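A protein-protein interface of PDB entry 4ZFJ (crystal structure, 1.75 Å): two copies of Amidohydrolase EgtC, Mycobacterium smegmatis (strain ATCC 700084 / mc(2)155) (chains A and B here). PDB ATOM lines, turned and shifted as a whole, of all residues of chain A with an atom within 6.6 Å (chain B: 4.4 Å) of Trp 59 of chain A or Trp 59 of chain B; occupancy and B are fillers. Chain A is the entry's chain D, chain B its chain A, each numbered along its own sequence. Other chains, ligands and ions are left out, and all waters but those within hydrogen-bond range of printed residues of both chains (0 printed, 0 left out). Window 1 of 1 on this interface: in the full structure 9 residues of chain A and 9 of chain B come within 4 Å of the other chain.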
ATOM      1  N   LEU A  14       3.319   4.687 -19.290  1.00  0.00           N
ATOM      2  CA  LEU A  14       2.847   5.024 -17.958  1.00  0.00           C
ATOM      3  C   LEU A  14       3.373   3.996 -16.965  1.00  0.00           C
ATOM      4  O   LEU A  14       3.745   4.349 -15.854  1.00  0.00           O
ATOM      5  CB  LEU A  14       1.319   5.085 -17.901  1.00  0.00           C
ATOM      6  CG  LEU A  14       0.614   6.162 -18.735  1.00  0.00           C
ATOM      7  CD1 LEU A  14      -0.883   6.136 -18.454  1.00  0.00           C
ATOM      8  CD2 LEU A  14       1.190   7.539 -18.475  1.00  0.00           C
ATOM      9  N   TRP A  45      -5.786   7.693  -7.194  1.00  0.00           N
ATOM     10  CA  TRP A  45      -4.637   7.998  -8.008  1.00  0.00           C
ATOM     11  C   TRP A  45      -5.141   8.528  -9.333  1.00  0.00           C
ATOM     12  O   TRP A  45      -6.331   8.439  -9.650  1.00  0.00           O
ATOM     13  CB  TRP A  45      -3.763   6.758  -8.233  1.00  0.00           C
ATOM     14  CG  TRP A  45      -4.520   5.633  -8.889  1.00  0.00           C
ATOM     15  CD1 TRP A  45      -5.241   4.663  -8.264  1.00  0.00           C
ATOM     16  CD2 TRP A  45      -4.641   5.379 -10.297  1.00  0.00           C
ATOM     17  NE1 TRP A  45      -5.807   3.823  -9.190  1.00  0.00           N
ATOM     18  CE2 TRP A  45      -5.454   4.242 -10.445  1.00  0.00           C
ATOM     19  CE3 TRP A  45      -4.149   6.007 -11.444  1.00  0.00           C
ATOM     20  CZ2 TRP A  45      -5.789   3.721 -11.693  1.00  0.00           C
ATOM     21  CZ3 TRP A  45      -4.480   5.482 -12.690  1.00  0.00           C
ATOM     22  CH2 TRP A  45      -5.294   4.357 -12.800  1.00  0.00           C
ATOM     23  N   GLY A  46      -4.230   9.088 -10.112  1.00  0.00           N
ATOM     24  CA  GLY A  46      -4.566   9.504 -11.449  1.00  0.00           C
ATOM     25  C   GLY A  46      -3.318   9.524 -12.292  1.00  0.00           C
ATOM     26  O   GLY A  46      -2.198   9.710 -11.785  1.00  0.00           O
ATOM     27  N   ALA A  47      -3.517   9.322 -13.585  1.00  0.00           N
ATOM     28  CA  ALA A  47      -2.448   9.421 -14.551  1.00  0.00           C
ATOM     29  C   ALA A  47      -2.985  10.172 -15.746  1.00  0.00           C
ATOM     30  O   ALA A  47      -3.981   9.761 -16.351  1.00  0.00           O
ATOM     31  CB  ALA A  47      -1.953   8.052 -14.951  1.00  0.00           C
ATOM     32  N   GLY A  48      -2.343  11.290 -16.047  1.00  0.00           N
ATOM     33  CA  GLY A  48      -2.664  12.081 -17.216  1.00  0.00           C
ATOM     34  C   GLY A  48      -1.505  12.085 -18.193  1.00  0.00           C
ATOM     35  O   GLY A  48      -0.336  12.032 -17.800  1.00  0.00           O
ATOM     36  N   PHE A  49      -1.829  12.150 -19.475  1.00  0.00           N
ATOM     37  CA  PHE A  49      -0.808  12.194 -20.505  1.00  0.00           C
ATOM     38  C   PHE A  49      -1.328  12.915 -21.728  1.00  0.00           C
ATOM     39  O   PHE A  49      -2.534  13.115 -21.876  1.00  0.00           O
ATOM     40  CB  PHE A  49      -0.347  10.781 -20.877  1.00  0.00           C
ATOM     41  CG  PHE A  49      -1.430   9.914 -21.470  1.00  0.00           C
ATOM     42  CD1 PHE A  49      -2.295   9.217 -20.651  1.00  0.00           C
ATOM     43  CD2 PHE A  49      -1.559   9.774 -22.844  1.00  0.00           C
ATOM     44  CE1 PHE A  49      -3.286   8.408 -21.186  1.00  0.00           C
ATOM     45  CE2 PHE A  49      -2.550   8.974 -23.386  1.00  0.00           C
ATOM     46  CZ  PHE A  49      -3.409   8.281 -22.549  1.00  0.00           C
ATOM     47  N   ARG A  57      -5.251  13.502 -21.919  1.00  0.00           N
ATOM     48  CA  ARG A  57      -6.072  12.354 -21.547  1.00  0.00           C
ATOM     49  C   ARG A  57      -5.767  11.951 -20.109  1.00  0.00           C
ATOM     50  O   ARG A  57      -4.636  12.108 -19.656  1.00  0.00           O
ATOM     51  CB  ARG A  57      -5.824  11.192 -22.512  1.00  0.00           C
ATOM     52  CG  ARG A  57      -6.061  11.603 -23.975  1.00  0.00           C
ATOM     53  CD  ARG A  57      -6.064  10.427 -24.956  1.00  0.00           C
ATOM     54  NE  ARG A  57      -6.316  10.929 -26.301  1.00  0.00           N
ATOM     55  CZ  ARG A  57      -7.512  11.268 -26.772  1.00  0.00           C
ATOM     56  NH1 ARG A  57      -8.601  11.134 -26.031  1.00  0.00           N
ATOM     57  NH2 ARG A  57      -7.621  11.739 -27.998  1.00  0.00           N
ATOM     58  N   ARG A  58      -6.778  11.442 -19.401  1.00  0.00           N
ATOM     59  CA  ARG A  58      -6.635  11.092 -17.992  1.00  0.00           C
ATOM     60  C   ARG A  58      -7.378   9.843 -17.576  1.00  0.00           C
ATOM     61  O   ARG A  58      -8.525   9.619 -17.978  1.00  0.00           O
ATOM     62  CB  ARG A  58      -7.158  12.220 -17.099  1.00  0.00           C
ATOM     63  CG  ARG A  58      -6.481  13.533 -17.206  1.00  0.00           C
ATOM     64  CD  ARG A  58      -7.135  14.508 -16.219  1.00  0.00           C
ATOM     65  NE  ARG A  58      -8.438  14.994 -16.657  1.00  0.00           N
ATOM     66  CZ  ARG A  58      -9.268  15.697 -15.889  1.00  0.00           C
ATOM     67  NH1 ARG A  58      -8.938  15.986 -14.635  1.00  0.00           N
ATOM     68  NH2 ARG A  58     -10.422  16.131 -16.375  1.00  0.00           N
ATOM     69  N   TRP A  59      -6.733   9.088 -16.694  1.00  0.00           N
ATOM     70  CA  TRP A  59      -7.323   7.938 -16.020  1.00  0.00           C
ATOM     71  C   TRP A  59      -7.258   8.233 -14.526  1.00  0.00           C
ATOM     72  O   TRP A  59      -6.170   8.474 -14.003  1.00  0.00           O
ATOM     73  CB  TRP A  59      -6.540   6.681 -16.392  1.00  0.00           C
ATOM     74  CG  TRP A  59      -7.078   5.365 -15.963  1.00  0.00           C
ATOM     75  CD1 TRP A  59      -7.968   5.101 -14.966  1.00  0.00           C
ATOM     76  CD2 TRP A  59      -6.726   4.103 -16.538  1.00  0.00           C
ATOM     77  NE1 TRP A  59      -8.196   3.741 -14.882  1.00  0.00           N
ATOM     78  CE2 TRP A  59      -7.444   3.108 -15.841  1.00  0.00           C
ATOM     79  CE3 TRP A  59      -5.878   3.720 -17.583  1.00  0.00           C
ATOM     80  CZ2 TRP A  59      -7.334   1.750 -16.156  1.00  0.00           C
ATOM     81  CZ3 TRP A  59      -5.765   2.377 -17.894  1.00  0.00           C
ATOM     82  CH2 TRP A  59      -6.493   1.410 -17.186  1.00  0.00           C
ATOM     83  N   ARG A  60      -8.404   8.273 -13.850  1.00  0.00           N
ATOM     84  CA  ARG A  60      -8.425   8.575 -12.424  1.00  0.00           C
ATOM     85  C   ARG A  60      -9.281   7.573 -11.668  1.00  0.00           C
ATOM     86  O   ARG A  60     -10.253   7.036 -12.204  1.00  0.00           O
ATOM     87  CB  ARG A  60      -8.936   9.994 -12.183  1.00  0.00           C
ATOM     88  CG  ARG A  60      -8.000  11.076 -12.727  1.00  0.00           C
ATOM     89  CD  ARG A  60      -8.377  12.436 -12.194  1.00  0.00           C
ATOM     90  NE  ARG A  60      -9.628  12.854 -12.785  1.00  0.00           N
ATOM     91  CZ  ARG A  60     -10.312  13.939 -12.444  1.00  0.00           C
ATOM     92  NH1 ARG A  60      -9.856  14.749 -11.498  1.00  0.00           N
ATOM     93  NH2 ARG A  60     -11.452  14.230 -13.058  1.00  0.00           N
ATOM     94  N   SER A  61      -8.917   7.352 -10.410  1.00  0.00           N
ATOM     95  CA  SER A  61      -9.571   6.360  -9.560  1.00  0.00           C
ATOM     96  C   SER A  61      -9.626   6.830  -8.112  1.00  0.00           C
ATOM     97  O   SER A  61      -8.850   7.699  -7.713  1.00  0.00           O
ATOM     98  CB  SER A  61      -8.822   5.038  -9.637  1.00  0.00           C
ATOM     99  OG  SER A  61      -9.351   4.109  -8.723  1.00  0.00           O
ATOM    100  N   ASP A  68      -5.149  -1.977  -8.600  1.00  0.00           N
ATOM    101  CA  ASP A  68      -5.855  -1.820  -9.869  1.00  0.00           C
ATOM    102  C   ASP A  68      -5.263  -2.717 -10.946  1.00  0.00           C
ATOM    103  O   ASP A  68      -4.215  -2.414 -11.531  1.00  0.00           O
ATOM    104  CB  ASP A  68      -5.842  -0.361 -10.327  1.00  0.00           C
ATOM    105  CG  ASP A  68      -6.900  -0.084 -11.374  1.00  0.00           C
ATOM    106  OD1 ASP A  68      -6.948  -0.832 -12.374  1.00  0.00           O
ATOM    107  OD2 ASP A  68      -7.704   0.853 -11.184  1.00  0.00           O
ATOM    108  N   SER A  70      -6.631  -3.471 -13.867  1.00  0.00           N
ATOM    109  CA  SER A  70      -6.797  -2.886 -15.208  1.00  0.00           C
ATOM    110  C   SER A  70      -5.635  -1.955 -15.538  1.00  0.00           C
ATOM    111  O   SER A  70      -5.077  -2.001 -16.635  1.00  0.00           O
ATOM    112  CB  SER A  70      -8.110  -2.101 -15.331  1.00  0.00           C
ATOM    113  OG  SER A  70      -9.240  -2.931 -15.300  1.00  0.00           O
ATOM    114  N   PHE A  71      -5.274  -1.075 -14.611  1.00  0.00           N
ATOM    115  CA  PHE A  71      -4.169  -0.168 -14.877  1.00  0.00           C
ATOM    116  C   PHE A  71      -2.870  -0.939 -15.038  1.00  0.00           C
ATOM    117  O   PHE A  71      -2.062  -0.621 -15.915  1.00  0.00           O
ATOM    118  CB  PHE A  71      -4.021   0.880 -13.769  1.00  0.00           C
ATOM    119  CG  PHE A  71      -3.036   1.969 -14.106  1.00  0.00           C
ATOM    120  CD1 PHE A  71      -3.288   2.851 -15.152  1.00  0.00           C
ATOM    121  CD2 PHE A  71      -1.869   2.116 -13.376  1.00  0.00           C
ATOM    122  CE1 PHE A  71      -2.384   3.862 -15.468  1.00  0.00           C
ATOM    123  CE2 PHE A  71      -0.961   3.131 -13.683  1.00  0.00           C
ATOM    124  CZ  PHE A  71      -1.218   4.002 -14.728  1.00  0.00           C
ATOM    125  N   ALA A  72      -2.657  -1.962 -14.217  1.00  0.00           N
ATOM    126  CA  ALA A  72      -1.428  -2.751 -14.333  1.00  0.00           C
ATOM    127  C   ALA A  72      -1.330  -3.433 -15.696  1.00  0.00           C
ATOM    128  O   ALA A  72      -0.240  -3.589 -16.229  1.00  0.00           O
ATOM    129  CB  ALA A  72      -1.336  -3.791 -13.231  1.00  0.00           C
ATOM    130  N   SER A  73      -2.476  -3.849 -16.241  1.00  0.00           N
ATOM    131  CA  SER A  73      -2.530  -4.534 -17.529  1.00  0.00           C
ATOM    132  C   SER A  73      -2.349  -3.566 -18.703  1.00  0.00           C
ATOM    133  O   SER A  73      -1.638  -3.863 -19.664  1.00  0.00           O
ATOM    134  CB  SER A  73      -3.861  -5.271 -17.687  1.00  0.00           C
ATOM    135  OG  SER A  73      -3.928  -5.947 -18.936  1.00  0.00           O
ATOM    136  N   VAL A  74      -3.015  -2.422 -18.625  1.00  0.00           N
ATOM    137  CA  VAL A  74      -3.070  -1.474 -19.746  1.00  0.00           C
ATOM    138  C   VAL A  74      -1.936  -0.440 -19.766  1.00  0.00           C
ATOM    139  O   VAL A  74      -1.505  -0.031 -20.842  1.00  0.00           O
ATOM    140  CB  VAL A  74      -4.430  -0.730 -19.739  1.00  0.00           C
ATOM    141  CG1 VAL A  74      -4.488   0.337 -20.831  1.00  0.00           C
ATOM    142  CG2 VAL A  74      -5.556  -1.726 -19.932  1.00  0.00           C
ATOM    143  N   ALA A  75      -1.458  -0.010 -18.598  1.00  0.00           N
ATOM    144  CA  ALA A  75      -0.451   1.056 -18.520  1.00  0.00           C
ATOM    145  C   ALA A  75       0.791   0.843 -19.412  1.00  0.00           C
ATOM    146  O   ALA A  75       1.346   1.816 -19.943  1.00  0.00           O
ATOM    147  CB  ALA A  75      -0.011   1.253 -17.056  1.00  0.00           C
ATOM    148  N   LEU A  78       0.280   2.365 -22.878  1.00  0.00           N
ATOM    149  CA  LEU A  78       0.053   3.803 -22.952  1.00  0.00           C
ATOM    150  C   LEU A  78       1.382   4.536 -22.850  1.00  0.00           C
ATOM    151  O   LEU A  78       2.019   4.523 -21.803  1.00  0.00           O
ATOM    152  CB  LEU A  78      -0.881   4.253 -21.840  1.00  0.00           C
ATOM    153  CG  LEU A  78      -2.335   3.809 -21.961  1.00  0.00           C
ATOM    154  CD1 LEU A  78      -3.038   4.128 -20.661  1.00  0.00           C
ATOM    155  CD2 LEU A  78      -3.018   4.486 -23.136  1.00  0.00           C
ATOM    156  N   ALA A 102      -5.885  14.046  -8.394  1.00  0.00           N
ATOM    157  CA  ALA A 102      -5.046  14.655  -9.416  1.00  0.00           C
ATOM    158  C   ALA A 102      -4.775  13.624 -10.507  1.00  0.00           C
ATOM    159  O   ALA A 102      -4.813  12.424 -10.235  1.00  0.00           O
ATOM    160  CB  ALA A 102      -3.756  15.146  -8.816  1.00  0.00           C
ATOM    161  N   PRO A 103      -4.482  14.073 -11.747  1.00  0.00           N
ATOM    162  CA  PRO A 103      -4.381  15.461 -12.207  1.00  0.00           C
ATOM    163  C   PRO A 103      -5.710  16.078 -12.624  1.00  0.00           C
ATOM    164  O   PRO A 103      -6.571  15.446 -13.238  1.00  0.00           O
ATOM    165  CB  PRO A 103      -3.448  15.364 -13.418  1.00  0.00           C
ATOM    166  CG  PRO A 103      -3.748  14.015 -14.004  1.00  0.00           C
ATOM    167  CD  PRO A 103      -4.107  13.117 -12.807  1.00  0.00           C
ATOM    168  N   TRP B  45     -18.484  -3.608 -17.765  1.00  0.00           N
ATOM    169  CA  TRP B  45     -18.017  -3.681 -19.134  1.00  0.00           C
ATOM    170  C   TRP B  45     -16.572  -4.135 -19.115  1.00  0.00           C
ATOM    171  O   TRP B  45     -15.928  -4.149 -18.068  1.00  0.00           O
ATOM    172  CB  TRP B  45     -18.135  -2.325 -19.851  1.00  0.00           C
ATOM    173  CG  TRP B  45     -17.335  -1.237 -19.195  1.00  0.00           C
ATOM    174  CD1 TRP B  45     -17.755  -0.394 -18.214  1.00  0.00           C
ATOM    175  CD2 TRP B  45     -15.965  -0.898 -19.453  1.00  0.00           C
ATOM    176  NE1 TRP B  45     -16.743   0.450 -17.845  1.00  0.00           N
ATOM    177  CE2 TRP B  45     -15.633   0.168 -18.593  1.00  0.00           C
ATOM    178  CE3 TRP B  45     -14.997  -1.385 -20.335  1.00  0.00           C
ATOM    179  CZ2 TRP B  45     -14.365   0.749 -18.578  1.00  0.00           C
ATOM    180  CZ3 TRP B  45     -13.735  -0.801 -20.327  1.00  0.00           C
ATOM    181  CH2 TRP B  45     -13.430   0.249 -19.444  1.00  0.00           C
ATOM    182  N   GLY B  46     -16.064  -4.497 -20.278  1.00  0.00           N
ATOM    183  CA  GLY B  46     -14.662  -4.842 -20.395  1.00  0.00           C
ATOM    184  C   GLY B  46     -14.176  -4.696 -21.816  1.00  0.00           C
ATOM    185  O   GLY B  46     -14.937  -4.838 -22.773  1.00  0.00           O
ATOM    186  N   ALA B  47     -12.897  -4.390 -21.945  1.00  0.00           N
ATOM    187  CA  ALA B  47     -12.260  -4.270 -23.250  1.00  0.00           C
ATOM    188  C   ALA B  47     -10.905  -4.951 -23.171  1.00  0.00           C
ATOM    189  O   ALA B  47     -10.088  -4.652 -22.287  1.00  0.00           O
ATOM    190  CB  ALA B  47     -12.127  -2.821 -23.659  1.00  0.00           C
ATOM    191  N   ARG B  58      -6.232  -6.166 -20.697  1.00  0.00           N
ATOM    192  CA  ARG B  58      -7.640  -5.989 -20.430  1.00  0.00           C
ATOM    193  C   ARG B  58      -7.899  -4.850 -19.455  1.00  0.00           C
ATOM    194  O   ARG B  58      -7.148  -4.656 -18.498  1.00  0.00           O
ATOM    195  CB  ARG B  58      -8.258  -7.249 -19.831  1.00  0.00           C
ATOM    196  CG  ARG B  58      -8.362  -8.440 -20.747  1.00  0.00           C
ATOM    197  CD  ARG B  58      -9.048  -9.598 -20.004  1.00  0.00           C
ATOM    198  NE  ARG B  58      -8.170 -10.230 -19.013  1.00  0.00           N
ATOM    199  CZ  ARG B  58      -8.562 -11.160 -18.136  1.00  0.00           C
ATOM    200  NH1 ARG B  58      -9.824 -11.555 -18.103  1.00  0.00           N
ATOM    201  NH2 ARG B  58      -7.700 -11.713 -17.288  1.00  0.00           N
ATOM    202  N   TRP B  59      -9.000  -4.166 -19.712  1.00  0.00           N
ATOM    203  CA  TRP B  59      -9.568  -3.147 -18.832  1.00  0.00           C
ATOM    204  C   TRP B  59     -10.996  -3.585 -18.539  1.00  0.00           C
ATOM    205  O   TRP B  59     -11.784  -3.733 -19.468  1.00  0.00           O
ATOM    206  CB  TRP B  59      -9.538  -1.794 -19.522  1.00  0.00           C
ATOM    207  CG  TRP B  59      -9.885  -0.598 -18.709  1.00  0.00           C
ATOM    208  CD1 TRP B  59     -10.573  -0.548 -17.540  1.00  0.00           C
ATOM    209  CD2 TRP B  59      -9.552   0.748 -19.044  1.00  0.00           C
ATOM    210  NE1 TRP B  59     -10.687   0.769 -17.113  1.00  0.00           N
ATOM    211  CE2 TRP B  59     -10.066   1.577 -18.032  1.00  0.00           C
ATOM    212  CE3 TRP B  59      -8.868   1.334 -20.112  1.00  0.00           C
ATOM    213  CZ2 TRP B  59      -9.912   2.960 -18.056  1.00  0.00           C
ATOM    214  CZ3 TRP B  59      -8.709   2.699 -20.129  1.00  0.00           C
ATOM    215  CH2 TRP B  59      -9.231   3.498 -19.115  1.00  0.00           C
ATOM    216  N   ARG B  60     -11.327  -3.818 -17.268  1.00  0.00           N
ATOM    217  CA  ARG B  60     -12.693  -4.205 -16.911  1.00  0.00           C
ATOM    218  C   ARG B  60     -13.206  -3.415 -15.735  1.00  0.00           C
ATOM    219  O   ARG B  60     -12.447  -2.964 -14.869  1.00  0.00           O
ATOM    220  CB  ARG B  60     -12.796  -5.689 -16.583  1.00  0.00           C
ATOM    221  CG  ARG B  60     -12.379  -6.584 -17.732  1.00  0.00           C
ATOM    222  CD  ARG B  60     -12.602  -8.048 -17.406  1.00  0.00           C
ATOM    223  NE  ARG B  60     -11.563  -8.526 -16.510  1.00  0.00           N
ATOM    224  CZ  ARG B  60     -11.568  -9.721 -15.939  1.00  0.00           C
ATOM    225  NH1 ARG B  60     -12.542 -10.600 -16.187  1.00  0.00           N
ATOM    226  NH2 ARG B  60     -10.575 -10.054 -15.130  1.00  0.00           N
ATOM    227  N   SER B  70     -12.917   7.893 -17.431  1.00  0.00           N
ATOM    228  CA  SER B  70     -11.532   7.507 -17.678  1.00  0.00           C
ATOM    229  C   SER B  70     -11.435   6.741 -18.996  1.00  0.00           C
ATOM    230  O   SER B  70     -10.571   7.018 -19.833  1.00  0.00           O
ATOM    231  CB  SER B  70     -10.986   6.654 -16.538  1.00  0.00           C
ATOM    232  OG  SER B  70     -10.808   7.415 -15.360  1.00  0.00           O
ATOM    233  N   PHE B  71     -12.320   5.776 -19.199  1.00  0.00           N
ATOM    234  CA  PHE B  71     -12.298   5.034 -20.464  1.00  0.00           C
ATOM    235  C   PHE B  71     -12.603   5.967 -21.644  1.00  0.00           C
ATOM    236  O   PHE B  71     -11.983   5.861 -22.700  1.00  0.00           O
ATOM    237  CB  PHE B  71     -13.278   3.862 -20.435  1.00  0.00           C
ATOM    238  CG  PHE B  71     -13.138   2.935 -21.607  1.00  0.00           C
ATOM    239  CD1 PHE B  71     -11.984   2.188 -21.775  1.00  0.00           C
ATOM    240  CD2 PHE B  71     -14.151   2.815 -22.537  1.00  0.00           C
ATOM    241  CE1 PHE B  71     -11.829   1.339 -22.854  1.00  0.00           C
ATOM    242  CE2 PHE B  71     -14.007   1.949 -23.636  1.00  0.00           C
ATOM    243  CZ  PHE B  71     -12.847   1.217 -23.787  1.00  0.00           C
ATOM    244  N   VAL B  74      -9.343   7.781 -22.354  1.00  0.00           N
ATOM    245  CA  VAL B  74      -8.130   7.051 -22.683  1.00  0.00           C
ATOM    246  C   VAL B  74      -8.314   6.129 -23.901  1.00  0.00           C
ATOM    247  O   VAL B  74      -7.357   5.859 -24.632  1.00  0.00           O
ATOM    248  CB  VAL B  74      -7.649   6.247 -21.446  1.00  0.00           C
ATOM    249  CG1 VAL B  74      -6.477   5.365 -21.782  1.00  0.00           C
ATOM    250  CG2 VAL B  74      -7.254   7.205 -20.310  1.00  0.00           C
ATOM    251  N   LEU B  78      -5.682   3.806 -27.309  1.00  0.00           N
ATOM    252  CA  LEU B  78      -5.411   2.370 -27.282  1.00  0.00           C
ATOM    253  C   LEU B  78      -5.841   1.760 -28.608  1.00  0.00           C
ATOM    254  O   LEU B  78      -7.030   1.666 -28.893  1.00  0.00           O
ATOM    255  CB  LEU B  78      -6.145   1.702 -26.128  1.00  0.00           C
ATOM    256  CG  LEU B  78      -5.678   2.127 -24.737  1.00  0.00           C
ATOM    257  CD1 LEU B  78      -6.674   1.686 -23.700  1.00  0.00           C
ATOM    258  CD2 LEU B  78      -4.311   1.545 -24.448  1.00  0.00           C
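The backbone NH of Ala 47 of chain A is in hydrogen-bond range of the backbone carbonyl oxygen of Trp 59 of chain A (2.8 Å).
The backbone carbonyl oxygen of Trp 59 of chain B is in hydrogen-bond range of the backbone NH of Ala 47 of chain B.
The side-chain carboxylate (OD1) of Asp 68 of chain A sits at hydrogen-bond distance from the backbone NH (N) of Ser 70 of chain A, 3.0 Å away.
NH1 of Arg 58 of chain A is in hydrogen-bond range of O of Pro 103 of chain A.
N of Leu 14 of chain A is in hydrogen-bond range of O of Leu 78 of chain A, 2.8 Å away.
Hydrophobic or aromatic side chains of chain A that line the printed part of chain B: Trp 59, Val 74 and Leu 78.
Among the printed residues, 13 pairs touch across the chains.
Printed residues of chain A within 4 Å of Trp 59 of chain B: Trp 59 and Ser 70.
Printed residues of chain B within 4 Å of Arg 60 of chain A: Ser 70 (3.0 Å).
Printed residues of chain B within 4 Å of Ser 70 of chain A: Arg 58, Trp 59 and Arg 60.
The nearest printed residue of chain B that does not touch Trp 59 of chain A is Val 74 of chain B (4.02 Å).
The nearest printed residue of chain B that does not touch Val 74 of chain A is Trp 59 of chain B (4.004 Å).
Among the printed residues, merely in contact across the chains: Trp 59 of chain A with Trp 59 of chain B (3.3 Å), Leu 78 of chain A with Leu 78 of chain B (3.5 Å), Ser 70 of chain A with Trp 59 of chain B (3.5 Å), Trp 59 of chain A with Ser 70 of chain B (3.6 Å), Arg 58 of chain A with Val 74 of chain B (3.6 Å), Val 74 of chain A with Arg 58 of chain B (3.6 Å), Arg 58 of chain A with Ser 70 of chain B (3.7 Å), Ser 70 of chain A with Arg 58 of chain B (3.8 Å), Leu 78 of chain A with Val 74 of chain B (3.8 Å) and Val 74 of chain A with Leu 78 of chain B (3.8 Å).
OG of Ser 70 of chain B sits at hydrogen-bond distance from N of Arg 60 of chain A.
The backbone NH (N) of Arg 58 of chain B is in hydrogen-bond range of the side-chain hydroxyl (OG) of Ser 73 of chain A (2.9 Å).
OG of Ser 70 of chain A is in hydrogen-bond range of N of Arg 60 of chain B (3.0 Å).
Arg 58 of chain A touches Ser 70 of chain B, and with the chains exchanged Ser 70 of chain A touches Arg 58 of chain B.
Trp 59 of chain A touches its own counterpart, Trp 59 of chain B.
Trp 59 of chain A touches Ser 70 of chain B, and with the chains exchanged Ser 70 of chain A touches Trp 59 of chain B.
Arg 60 of chain A touches Ser 70 of chain B, and with the chains exchanged Ser 70 of chain A touches Arg 60 of chain B.
10 positions are printed for both chains.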
